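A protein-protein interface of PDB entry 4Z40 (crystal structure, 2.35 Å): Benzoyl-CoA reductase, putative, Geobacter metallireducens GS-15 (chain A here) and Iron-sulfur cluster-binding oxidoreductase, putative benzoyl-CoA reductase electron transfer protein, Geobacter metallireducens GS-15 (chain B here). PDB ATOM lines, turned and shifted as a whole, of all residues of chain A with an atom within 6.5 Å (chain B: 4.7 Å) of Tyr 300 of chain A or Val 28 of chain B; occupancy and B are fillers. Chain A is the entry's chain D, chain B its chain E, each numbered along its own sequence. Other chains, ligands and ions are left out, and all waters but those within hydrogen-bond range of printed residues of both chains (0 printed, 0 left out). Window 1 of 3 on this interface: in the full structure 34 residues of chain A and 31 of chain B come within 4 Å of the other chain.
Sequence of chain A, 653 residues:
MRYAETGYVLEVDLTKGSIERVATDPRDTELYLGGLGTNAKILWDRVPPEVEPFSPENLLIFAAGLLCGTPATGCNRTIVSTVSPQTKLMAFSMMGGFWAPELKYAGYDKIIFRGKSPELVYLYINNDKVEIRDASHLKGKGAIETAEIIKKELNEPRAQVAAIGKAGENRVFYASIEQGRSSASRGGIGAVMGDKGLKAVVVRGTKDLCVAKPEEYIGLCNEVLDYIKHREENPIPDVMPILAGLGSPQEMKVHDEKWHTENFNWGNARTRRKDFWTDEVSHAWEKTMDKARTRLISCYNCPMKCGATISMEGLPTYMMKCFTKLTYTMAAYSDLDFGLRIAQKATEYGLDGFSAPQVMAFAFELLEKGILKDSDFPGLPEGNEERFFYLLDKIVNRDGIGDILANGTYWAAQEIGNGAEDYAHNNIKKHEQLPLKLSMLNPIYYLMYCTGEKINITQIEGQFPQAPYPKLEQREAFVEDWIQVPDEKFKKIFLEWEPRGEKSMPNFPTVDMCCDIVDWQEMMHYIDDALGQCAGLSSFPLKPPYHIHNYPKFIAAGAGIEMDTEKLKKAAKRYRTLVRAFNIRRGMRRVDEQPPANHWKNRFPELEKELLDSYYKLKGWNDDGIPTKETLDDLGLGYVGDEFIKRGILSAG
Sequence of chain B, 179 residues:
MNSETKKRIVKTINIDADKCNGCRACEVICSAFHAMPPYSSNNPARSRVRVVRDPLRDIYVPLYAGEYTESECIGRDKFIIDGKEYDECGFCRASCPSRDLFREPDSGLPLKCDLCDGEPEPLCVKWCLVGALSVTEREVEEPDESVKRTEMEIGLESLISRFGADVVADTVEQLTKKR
The backbone NH (N) of Asn 301 of chain A is in hydrogen-bond range of the backbone carbonyl oxygen (O) of Cys 23 of chain B (2.8 Å).
The backbone carbonyl oxygen (O) of Gly 69 of chain A lies within hydrogen-bond range of the side-chain amide nitrogen (ND2) of Asn 42 of chain B.
OH of Tyr 105 of chain A is in hydrogen-bond range of OD1 of Asn 42 of chain B.
O of Gly 97 of chain A sits at hydrogen-bond distance from N of Tyr 300 of chain A, 3.1 Å away.
The backbone carbonyl oxygen (O) of Val 28 of chain B is in hydrogen-bond range of the side-chain hydroxyl (OG) of Ser 31 of chain B (2.9 Å).
SG of Cys 299 of chain A lies close to NH1 of Arg 77 of chain A (3.5 Å).
ND2 of Asn 301 of chain A is in hydrogen-bond range of O of Ala 72 of chain A, at 3.3 Å.
N of Ala 25 of chain B sits close to SG of Cys 23 of chain B (3.4 Å).
The side-chain carboxylate of Glu 27 of chain B is in salt-bridge range of the guanidinium group of Arg 24 of chain B, 3.1 Å away.
ND2 of Asn 42 of chain B touches CA of Thr 70 of chain A (3.6 Å).
Pro 71 of chain A touches Val 28 of chain B (CA to CG1, 3.9 Å).
CD of Pro 71 of chain A touches ND2 of Asn 42 of chain B (3.4 Å).
CE2 of Phe 98 of chain A touches O of Cys 23 of chain B, at 3.9 Å.
Phe 98 of chain A touches Arg 24 of chain B.
Tyr 105 of chain A touches Pro 44 of chain B.
CB of Ser 298 of chain A touches CB of Cys 23 of chain B, 3.7 Å away.
Arg 24 of chain B touches Tyr 300 of chain A (CZ to CE1, 3.7 Å).
Val 28 of chain B touches Tyr 300 of chain A.
Cys 302 of chain A touches Cys 23 of chain B (O to CB, 3.2 Å).
Of the printed residues of chain B, Gly 69 of chain A touches Asn 42 (2.9 Å).
Gly 96 of chain A touches none of the printed residues of chain B.
Printed residues of chain B within 4 Å of Phe 98 of chain A: Cys 23 (3.9 Å) and Arg 24 (3.6 Å).
Of chain B, only Cys 23, Arg 24, Val 28 and Pro 44 come within 4 Å of Tyr 300 of chain A.
Cys 26 of chain B touches none of the printed residues of chain A.
Of the printed residues of chain A, Asn 42 of chain B touches Gly 69 (2.9 Å), Thr 70 (3.6 Å), Pro 71 (3.4 Å) and Tyr 105 (2.7 Å).
Printed residues of chain A within 4 Å of Pro 44 of chain B: Tyr 105 and Tyr 300.
The nearest residue of chain B that does not touch Tyr 300 of chain A is Asn 42 of chain B (4.6 Å).
The nearest printed residue of chain B that does not touch Tyr 105 of chain A is Val 28 of chain B (4.8 Å).
Of the 12 printed residues of chain B, 6 touch a printed residue of chain A.
Printed residues of chain B that touch a printed residue of chain A: Cys 23, Arg 24, Ala 25, Val 28, Asn 42 and Pro 44.
Hydrophobic or aromatic side chains of chain B that line the printed part of chain A: Ala 25, Val 28 and Pro 44.
Of the 21 printed residues of chain A, 10 touch a printed residue of chain B.
Hydrophobic or aromatic side chains of chain A within 4 Å of the printed part of chain B: Pro 71, Phe 98, Tyr 105 and Tyr 300.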
ATOM      1  N   GLY A  69       2.836  24.955  -4.256  1.00  0.00           N
ATOM      2  CA  GLY A  69       3.992  24.701  -3.421  1.00  0.00           C
ATOM      3  C   GLY A  69       5.019  25.813  -3.483  1.00  0.00           C
ATOM      4  O   GLY A  69       6.048  25.745  -2.816  1.00  0.00           O
ATOM      5  N   THR A  70       4.743  26.832  -4.289  1.00  0.00           N
ATOM      6  CA  THR A  70       5.579  28.030  -4.335  1.00  0.00           C
ATOM      7  C   THR A  70       4.925  29.103  -3.465  1.00  0.00           C
ATOM      8  O   THR A  70       3.777  28.937  -3.048  1.00  0.00           O
ATOM      9  CB  THR A  70       5.758  28.564  -5.785  1.00  0.00           C
ATOM     10  OG1 THR A  70       4.526  29.130  -6.248  1.00  0.00           O
ATOM     11  CG2 THR A  70       6.208  27.457  -6.728  1.00  0.00           C
ATOM     12  N   PRO A  71       5.640  30.202  -3.180  1.00  0.00           N
ATOM     13  CA  PRO A  71       5.020  31.254  -2.366  1.00  0.00           C
ATOM     14  C   PRO A  71       3.833  31.983  -3.020  1.00  0.00           C
ATOM     15  O   PRO A  71       3.257  32.867  -2.386  1.00  0.00           O
ATOM     16  CB  PRO A  71       6.174  32.234  -2.135  1.00  0.00           C
ATOM     17  CG  PRO A  71       7.391  31.399  -2.221  1.00  0.00           C
ATOM     18  CD  PRO A  71       7.093  30.404  -3.306  1.00  0.00           C
ATOM     19  N   ALA A  72       3.475  31.630  -4.253  1.00  0.00           N
ATOM     20  CA  ALA A  72       2.391  32.314  -4.963  1.00  0.00           C
ATOM     21  C   ALA A  72       1.061  32.219  -4.217  1.00  0.00           C
ATOM     22  O   ALA A  72       0.511  31.130  -4.044  1.00  0.00           O
ATOM     23  CB  ALA A  72       2.243  31.753  -6.356  1.00  0.00           C
ATOM     24  N   THR A  73       0.555  33.371  -3.788  1.00  0.00           N
ATOM     25  CA  THR A  73      -0.700  33.464  -3.049  1.00  0.00           C
ATOM     26  C   THR A  73      -1.850  32.707  -3.714  1.00  0.00           C
ATOM     27  O   THR A  73      -2.131  32.902  -4.900  1.00  0.00           O
ATOM     28  CB  THR A  73      -1.127  34.928  -2.890  1.00  0.00           C
ATOM     29  OG1 THR A  73      -0.042  35.693  -2.350  1.00  0.00           O
ATOM     30  CG2 THR A  73      -2.343  35.030  -1.982  1.00  0.00           C
ATOM     31  N   GLY A  74      -2.507  31.847  -2.947  1.00  0.00           N
ATOM     32  CA  GLY A  74      -3.679  31.135  -3.413  1.00  0.00           C
ATOM     33  C   GLY A  74      -3.414  30.077  -4.466  1.00  0.00           C
ATOM     34  O   GLY A  74      -4.348  29.603  -5.120  1.00  0.00           O
ATOM     35  N   CYS A  75      -2.152  29.693  -4.641  1.00  0.00           N
ATOM     36  CA  CYS A  75      -1.824  28.697  -5.657  1.00  0.00           C
ATOM     37  C   CYS A  75      -1.761  27.295  -5.063  1.00  0.00           C
ATOM     38  O   CYS A  75      -0.710  26.856  -4.628  1.00  0.00           O
ATOM     39  CB  CYS A  75      -0.501  29.036  -6.334  1.00  0.00           C
ATOM     40  SG  CYS A  75      -0.324  28.241  -7.937  1.00  0.00           S
ATOM     41  N   ASN A  76      -2.880  26.581  -5.091  1.00  0.00           N
ATOM     42  CA  ASN A  76      -3.023  25.388  -4.267  1.00  0.00           C
ATOM     43  C   ASN A  76      -3.990  24.343  -4.814  1.00  0.00           C
ATOM     44  O   ASN A  76      -4.350  23.391  -4.136  1.00  0.00           O
ATOM     45  CB  ASN A  76      -3.480  25.824  -2.877  1.00  0.00           C
ATOM     46  CG  ASN A  76      -4.669  26.766  -2.943  1.00  0.00           C
ATOM     47  OD1 ASN A  76      -5.581  26.558  -3.740  1.00  0.00           O
ATOM     48  ND2 ASN A  76      -4.650  27.820  -2.139  1.00  0.00           N
ATOM     49  N   ARG A  77      -4.418  24.507  -6.051  1.00  0.00           N
ATOM     50  CA  ARG A  77      -5.480  23.649  -6.570  1.00  0.00           C
ATOM     51  C   ARG A  77      -4.977  22.285  -7.043  1.00  0.00           C
ATOM     52  O   ARG A  77      -3.939  22.180  -7.697  1.00  0.00           O
ATOM     53  CB  ARG A  77      -6.220  24.366  -7.703  1.00  0.00           C
ATOM     54  CG  ARG A  77      -7.650  24.791  -7.340  1.00  0.00           C
ATOM     55  CD  ARG A  77      -7.693  25.810  -6.204  1.00  0.00           C
ATOM     56  NE  ARG A  77      -9.037  25.911  -5.636  1.00  0.00           N
ATOM     57  CZ  ARG A  77      -9.355  26.607  -4.546  1.00  0.00           C
ATOM     58  NH1 ARG A  77      -8.415  27.270  -3.887  1.00  0.00           N
ATOM     59  NH2 ARG A  77     -10.616  26.627  -4.113  1.00  0.00           N
ATOM     60  N   GLY A  96      -9.543  22.766  -3.966  1.00  0.00           N
ATOM     61  CA  GLY A  96      -8.631  23.652  -3.266  1.00  0.00           C
ATOM     62  C   GLY A  96      -8.063  23.050  -1.992  1.00  0.00           C
ATOM     63  O   GLY A  96      -7.804  21.846  -1.913  1.00  0.00           O
ATOM     64  N   GLY A  97      -7.872  23.898  -0.991  1.00  0.00           N
ATOM     65  CA  GLY A  97      -7.372  23.460   0.303  1.00  0.00           C
ATOM     66  C   GLY A  97      -5.868  23.296   0.386  1.00  0.00           C
ATOM     67  O   GLY A  97      -5.120  24.208   0.028  1.00  0.00           O
ATOM     68  N   PHE A  98      -5.429  22.126   0.855  1.00  0.00           N
ATOM     69  CA  PHE A  98      -4.037  21.954   1.261  1.00  0.00           C
ATOM     70  C   PHE A  98      -3.404  20.710   0.655  1.00  0.00           C
ATOM     71  O   PHE A  98      -2.259  20.394   0.944  1.00  0.00           O
ATOM     72  CB  PHE A  98      -3.930  21.904   2.805  1.00  0.00           C
ATOM     73  CG  PHE A  98      -4.397  23.164   3.489  1.00  0.00           C
ATOM     74  CD1 PHE A  98      -5.746  23.417   3.669  1.00  0.00           C
ATOM     75  CD2 PHE A  98      -3.489  24.104   3.925  1.00  0.00           C
ATOM     76  CE1 PHE A  98      -6.176  24.586   4.270  1.00  0.00           C
ATOM     77  CE2 PHE A  98      -3.913  25.280   4.535  1.00  0.00           C
ATOM     78  CZ  PHE A  98      -5.255  25.517   4.711  1.00  0.00           C
ATOM     79  N   TRP A  99      -4.134  20.015  -0.210  1.00  0.00           N
ATOM     80  CA  TRP A  99      -3.679  18.703  -0.668  1.00  0.00           C
ATOM     81  C   TRP A  99      -2.613  18.783  -1.765  1.00  0.00           C
ATOM     82  O   TRP A  99      -1.592  18.102  -1.686  1.00  0.00           O
ATOM     83  CB  TRP A  99      -4.862  17.876  -1.132  1.00  0.00           C
ATOM     84  CG  TRP A  99      -4.545  16.434  -1.339  1.00  0.00           C
ATOM     85  CD1 TRP A  99      -4.710  15.430  -0.440  1.00  0.00           C
ATOM     86  CD2 TRP A  99      -4.018  15.829  -2.525  1.00  0.00           C
ATOM     87  NE1 TRP A  99      -4.307  14.239  -0.978  1.00  0.00           N
ATOM     88  CE2 TRP A  99      -3.888  14.451  -2.264  1.00  0.00           C
ATOM     89  CE3 TRP A  99      -3.662  16.315  -3.787  1.00  0.00           C
ATOM     90  CZ2 TRP A  99      -3.398  13.547  -3.217  1.00  0.00           C
ATOM     91  CZ3 TRP A  99      -3.175  15.415  -4.736  1.00  0.00           C
ATOM     92  CH2 TRP A  99      -3.038  14.047  -4.435  1.00  0.00           C
ATOM     93  N   PRO A 101      -0.381  21.269  -2.606  1.00  0.00           N
ATOM     94  CA  PRO A 101       0.958  21.655  -2.136  1.00  0.00           C
ATOM     95  C   PRO A 101       1.691  20.533  -1.379  1.00  0.00           C
ATOM     96  O   PRO A 101       2.908  20.375  -1.539  1.00  0.00           O
ATOM     97  CB  PRO A 101       0.669  22.836  -1.201  1.00  0.00           C
ATOM     98  CG  PRO A 101      -0.604  23.406  -1.723  1.00  0.00           C
ATOM     99  CD  PRO A 101      -1.409  22.214  -2.126  1.00  0.00           C
ATOM    100  N   GLU A 102       0.960  19.770  -0.570  1.00  0.00           N
ATOM    101  CA  GLU A 102       1.579  18.702   0.211  1.00  0.00           C
ATOM    102  C   GLU A 102       2.214  17.678  -0.735  1.00  0.00           C
ATOM    103  O   GLU A 102       3.314  17.175  -0.479  1.00  0.00           O
ATOM    104  CB  GLU A 102       0.550  18.036   1.131  1.00  0.00           C
ATOM    105  CG  GLU A 102       1.133  17.102   2.151  1.00  0.00           C
ATOM    106  CD  GLU A 102       1.775  17.834   3.339  1.00  0.00           C
ATOM    107  OE1 GLU A 102       2.507  17.169   4.111  1.00  0.00           O
ATOM    108  OE2 GLU A 102       1.544  19.059   3.505  1.00  0.00           O
ATOM    109  N   TYR A 105       5.419  18.998  -1.896  1.00  0.00           N
ATOM    110  CA  TYR A 105       6.412  18.914  -0.822  1.00  0.00           C
ATOM    111  C   TYR A 105       6.823  17.459  -0.615  1.00  0.00           C
ATOM    112  O   TYR A 105       7.879  17.182  -0.051  1.00  0.00           O
ATOM    113  CB  TYR A 105       5.876  19.507   0.490  1.00  0.00           C
ATOM    114  CG  TYR A 105       5.618  20.997   0.450  1.00  0.00           C
ATOM    115  CD1 TYR A 105       6.591  21.884   0.007  1.00  0.00           C
ATOM    116  CD2 TYR A 105       4.392  21.518   0.851  1.00  0.00           C
ATOM    117  CE1 TYR A 105       6.345  23.255  -0.036  1.00  0.00           C
ATOM    118  CE2 TYR A 105       4.135  22.879   0.805  1.00  0.00           C
ATOM    119  CZ  TYR A 105       5.112  23.738   0.365  1.00  0.00           C
ATOM    120  OH  TYR A 105       4.836  25.082   0.327  1.00  0.00           O
ATOM    121  N   SER A 298      -9.355  29.888   5.373  1.00  0.00           N
ATOM    122  CA  SER A 298      -8.733  29.963   4.053  1.00  0.00           C
ATOM    123  C   SER A 298      -8.183  28.648   3.508  1.00  0.00           C
ATOM    124  O   SER A 298      -7.867  27.723   4.272  1.00  0.00           O
ATOM    125  CB  SER A 298      -7.582  30.965   4.099  1.00  0.00           C
ATOM    126  OG  SER A 298      -8.033  32.289   4.319  1.00  0.00           O
ATOM    127  N   CYS A 299      -8.024  28.583   2.185  1.00  0.00           N
ATOM    128  CA  CYS A 299      -7.189  27.554   1.575  1.00  0.00           C
ATOM    129  C   CYS A 299      -5.712  27.872   1.855  1.00  0.00           C
ATOM    130  O   CYS A 299      -5.404  28.910   2.440  1.00  0.00           O
ATOM    131  CB  CYS A 299      -7.437  27.462   0.066  1.00  0.00           C
ATOM    132  SG  CYS A 299      -9.153  27.187  -0.429  1.00  0.00           S
ATOM    133  N   TYR A 300      -4.805  26.999   1.430  1.00  0.00           N
ATOM    134  CA  TYR A 300      -3.370  27.207   1.650  1.00  0.00           C
ATOM    135  C   TYR A 300      -2.863  28.524   1.078  1.00  0.00           C
ATOM    136  O   TYR A 300      -3.130  28.845  -0.081  1.00  0.00           O
ATOM    137  CB  TYR A 300      -2.577  26.055   1.040  1.00  0.00           C
ATOM    138  CG  TYR A 300      -1.098  26.038   1.368  1.00  0.00           C
ATOM    139  CD1 TYR A 300      -0.639  25.879   2.695  1.00  0.00           C
ATOM    140  CD2 TYR A 300      -0.153  26.129   0.357  1.00  0.00           C
ATOM    141  CE1 TYR A 300       0.720  25.847   2.984  1.00  0.00           C
ATOM    142  CE2 TYR A 300       1.208  26.083   0.631  1.00  0.00           C
ATOM    143  CZ  TYR A 300       1.640  25.944   1.950  1.00  0.00           C
ATOM    144  OH  TYR A 300       2.996  25.910   2.221  1.00  0.00           O
ATOM    145  N   ASN A 301      -2.150  29.284   1.908  1.00  0.00           N
ATOM    146  CA  ASN A 301      -1.477  30.510   1.482  1.00  0.00           C
ATOM    147  C   ASN A 301      -2.416  31.533   0.810  1.00  0.00           C
ATOM    148  O   ASN A 301      -2.102  32.078  -0.250  1.00  0.00           O
ATOM    149  CB  ASN A 301      -0.317  30.158   0.540  1.00  0.00           C
ATOM    150  CG  ASN A 301       0.614  31.327   0.300  1.00  0.00           C
ATOM    151  OD1 ASN A 301       0.735  32.217   1.149  1.00  0.00           O
ATOM    152  ND2 ASN A 301       1.270  31.342  -0.858  1.00  0.00           N
ATOM    153  N   CYS A 302      -3.559  31.797   1.441  1.00  0.00           N
ATOM    154  CA  CYS A 302      -4.510  32.789   0.942  1.00  0.00           C
ATOM    155  C   CYS A 302      -5.211  33.538   2.073  1.00  0.00           C
ATOM    156  O   CYS A 302      -5.652  32.937   3.046  1.00  0.00           O
ATOM    157  CB  CYS A 302      -5.559  32.124   0.054  1.00  0.00           C
ATOM    158  SG  CYS A 302      -6.651  33.297  -0.843  1.00  0.00           S
ATOM    159  N   CYS B  23      -4.475  29.727   7.106  1.00  0.00           N
ATOM    160  CA  CYS B  23      -3.948  29.719   5.745  1.00  0.00           C
ATOM    161  C   CYS B  23      -2.513  29.192   5.662  1.00  0.00           C
ATOM    162  O   CYS B  23      -2.079  28.729   4.602  1.00  0.00           O
ATOM    163  CB  CYS B  23      -4.011  31.128   5.150  1.00  0.00           C
ATOM    164  SG  CYS B  23      -2.796  32.269   5.814  1.00  0.00           S
ATOM    165  N   ARG B  24      -1.790  29.286   6.779  1.00  0.00           N
ATOM    166  CA  ARG B  24      -0.412  28.810   6.892  1.00  0.00           C
ATOM    167  C   ARG B  24       0.584  29.591   6.014  1.00  0.00           C
ATOM    168  O   ARG B  24       1.667  29.084   5.701  1.00  0.00           O
ATOM    169  CB  ARG B  24      -0.348  27.306   6.573  1.00  0.00           C
ATOM    170  CG  ARG B  24      -1.113  26.435   7.584  1.00  0.00           C
ATOM    171  CD  ARG B  24      -1.003  24.939   7.296  1.00  0.00           C
ATOM    172  NE  ARG B  24       0.343  24.561   6.864  1.00  0.00           N
ATOM    173  CZ  ARG B  24       0.597  23.613   5.965  1.00  0.00           C
ATOM    174  NH1 ARG B  24      -0.413  22.930   5.416  1.00  0.00           N
ATOM    175  NH2 ARG B  24       1.858  23.346   5.618  1.00  0.00           N
ATOM    176  N   ALA B  25       0.235  30.830   5.660  1.00  0.00           N
ATOM    177  CA  ALA B  25       1.101  31.688   4.847  1.00  0.00           C
ATOM    178  C   ALA B  25       2.381  32.085   5.578  1.00  0.00           C
ATOM    179  O   ALA B  25       3.463  32.117   4.979  1.00  0.00           O
ATOM    180  CB  ALA B  25       0.352  32.942   4.410  1.00  0.00           C
ATOM    181  N   CYS B  26       2.244  32.423   6.859  1.00  0.00           N
ATOM    182  CA  CYS B  26       3.399  32.651   7.730  1.00  0.00           C
ATOM    183  C   CYS B  26       4.440  31.547   7.577  1.00  0.00           C
ATOM    184  O   CYS B  26       5.632  31.828   7.404  1.00  0.00           O
ATOM    185  CB  CYS B  26       2.950  32.746   9.188  1.00  0.00           C
ATOM    186  SG  CYS B  26       1.636  31.596   9.558  1.00  0.00           S
ATOM    187  N   GLU B  27       3.973  30.297   7.612  1.00  0.00           N
ATOM    188  CA  GLU B  27       4.854  29.132   7.484  1.00  0.00           C
ATOM    189  C   GLU B  27       5.625  29.166   6.171  1.00  0.00           C
ATOM    190  O   GLU B  27       6.819  28.859   6.132  1.00  0.00           O
ATOM    191  CB  GLU B  27       4.062  27.821   7.579  1.00  0.00           C
ATOM    192  CG  GLU B  27       3.519  27.465   8.964  1.00  0.00           C
ATOM    193  CD  GLU B  27       3.017  26.026   9.014  1.00  0.00           C
ATOM    194  OE1 GLU B  27       3.129  25.339   7.980  1.00  0.00           O
ATOM    195  OE2 GLU B  27       2.523  25.574  10.076  1.00  0.00           O
ATOM    196  N   VAL B  28       4.926  29.563   5.110  1.00  0.00           N
ATOM    197  CA  VAL B  28       5.489  29.648   3.772  1.00  0.00           C
ATOM    198  C   VAL B  28       6.594  30.680   3.646  1.00  0.00           C
ATOM    199  O   VAL B  28       7.673  30.393   3.125  1.00  0.00           O
ATOM    200  CB  VAL B  28       4.396  30.006   2.731  1.00  0.00           C
ATOM    201  CG1 VAL B  28       5.011  30.224   1.359  1.00  0.00           C
ATOM    202  CG2 VAL B  28       3.324  28.940   2.700  1.00  0.00           C
ATOM    203  N   ILE B  29       6.298  31.896   4.088  1.00  0.00           N
ATOM    204  CA  ILE B  29       7.214  33.008   3.882  1.00  0.00           C
ATOM    205  C   ILE B  29       8.432  32.892   4.794  1.00  0.00           C
ATOM    206  O   ILE B  29       9.529  33.271   4.385  1.00  0.00           O
ATOM    207  CB  ILE B  29       6.514  34.386   4.095  1.00  0.00           C
ATOM    208  CG1 ILE B  29       7.412  35.542   3.646  1.00  0.00           C
ATOM    209  CG2 ILE B  29       6.128  34.595   5.555  1.00  0.00           C
ATOM    210  CD1 ILE B  29       8.000  35.386   2.264  1.00  0.00           C
ATOM    211  N   CYS B  30       8.264  32.348   6.006  1.00  0.00           N
ATOM    212  CA  CYS B  30       9.394  32.226   6.946  1.00  0.00           C
ATOM    213  C   CYS B  30      10.384  31.190   6.429  1.00  0.00           C
ATOM    214  O   CYS B  30      11.585  31.430   6.425  1.00  0.00           O
ATOM    215  CB  CYS B  30       8.920  31.852   8.367  1.00  0.00           C
ATOM    216  SG  CYS B  30      10.238  31.418   9.577  1.00  0.00           S
ATOM    217  N   SER B  31       9.878  30.046   5.973  1.00  0.00           N
ATOM    218  CA  SER B  31      10.757  29.032   5.394  1.00  0.00           C
ATOM    219  C   SER B  31      11.443  29.574   4.152  1.00  0.00           C
ATOM    220  O   SER B  31      12.646  29.372   3.963  1.00  0.00           O
ATOM    221  CB  SER B  31       9.989  27.754   5.053  1.00  0.00           C
ATOM    222  OG  SER B  31       8.801  28.025   4.342  1.00  0.00           O
ATOM    223  N   ALA B  32      10.680  30.283   3.324  1.00  0.00           N
ATOM    224  CA  ALA B  32      11.215  30.832   2.085  1.00  0.00           C
ATOM    225  C   ALA B  32      12.325  31.835   2.379  1.00  0.00           C
ATOM    226  O   ALA B  32      13.372  31.807   1.735  1.00  0.00           O
ATOM    227  CB  ALA B  32      10.103  31.477   1.247  1.00  0.00           C
ATOM    228  N   ASN B  42      10.976  26.831  -0.562  1.00  0.00           N
ATOM    229  CA  ASN B  42      10.253  26.898   0.697  1.00  0.00           C
ATOM    230  C   ASN B  42       9.862  25.503   1.157  1.00  0.00           C
ATOM    231  O   ASN B  42       9.982  24.531   0.402  1.00  0.00           O
ATOM    232  CB  ASN B  42       9.032  27.817   0.595  1.00  0.00           C
ATOM    233  CG  ASN B  42       7.913  27.225  -0.228  1.00  0.00           C
ATOM    234  OD1 ASN B  42       7.135  26.413   0.272  1.00  0.00           O
ATOM    235  ND2 ASN B  42       7.802  27.651  -1.491  1.00  0.00           N
ATOM    236  N   PRO B  44       7.439  24.283   4.701  1.00  0.00           N
ATOM    237  CA  PRO B  44       6.779  24.497   5.994  1.00  0.00           C
ATOM    238  C   PRO B  44       7.447  23.763   7.166  1.00  0.00           C
ATOM    239  O   PRO B  44       7.461  24.287   8.288  1.00  0.00           O
ATOM    240  CB  PRO B  44       5.365  23.969   5.739  1.00  0.00           C
ATOM    241  CG  PRO B  44       5.127  24.278   4.290  1.00  0.00           C
ATOM    242  CD  PRO B  44       6.466  24.129   3.600  1.00  0.00           C
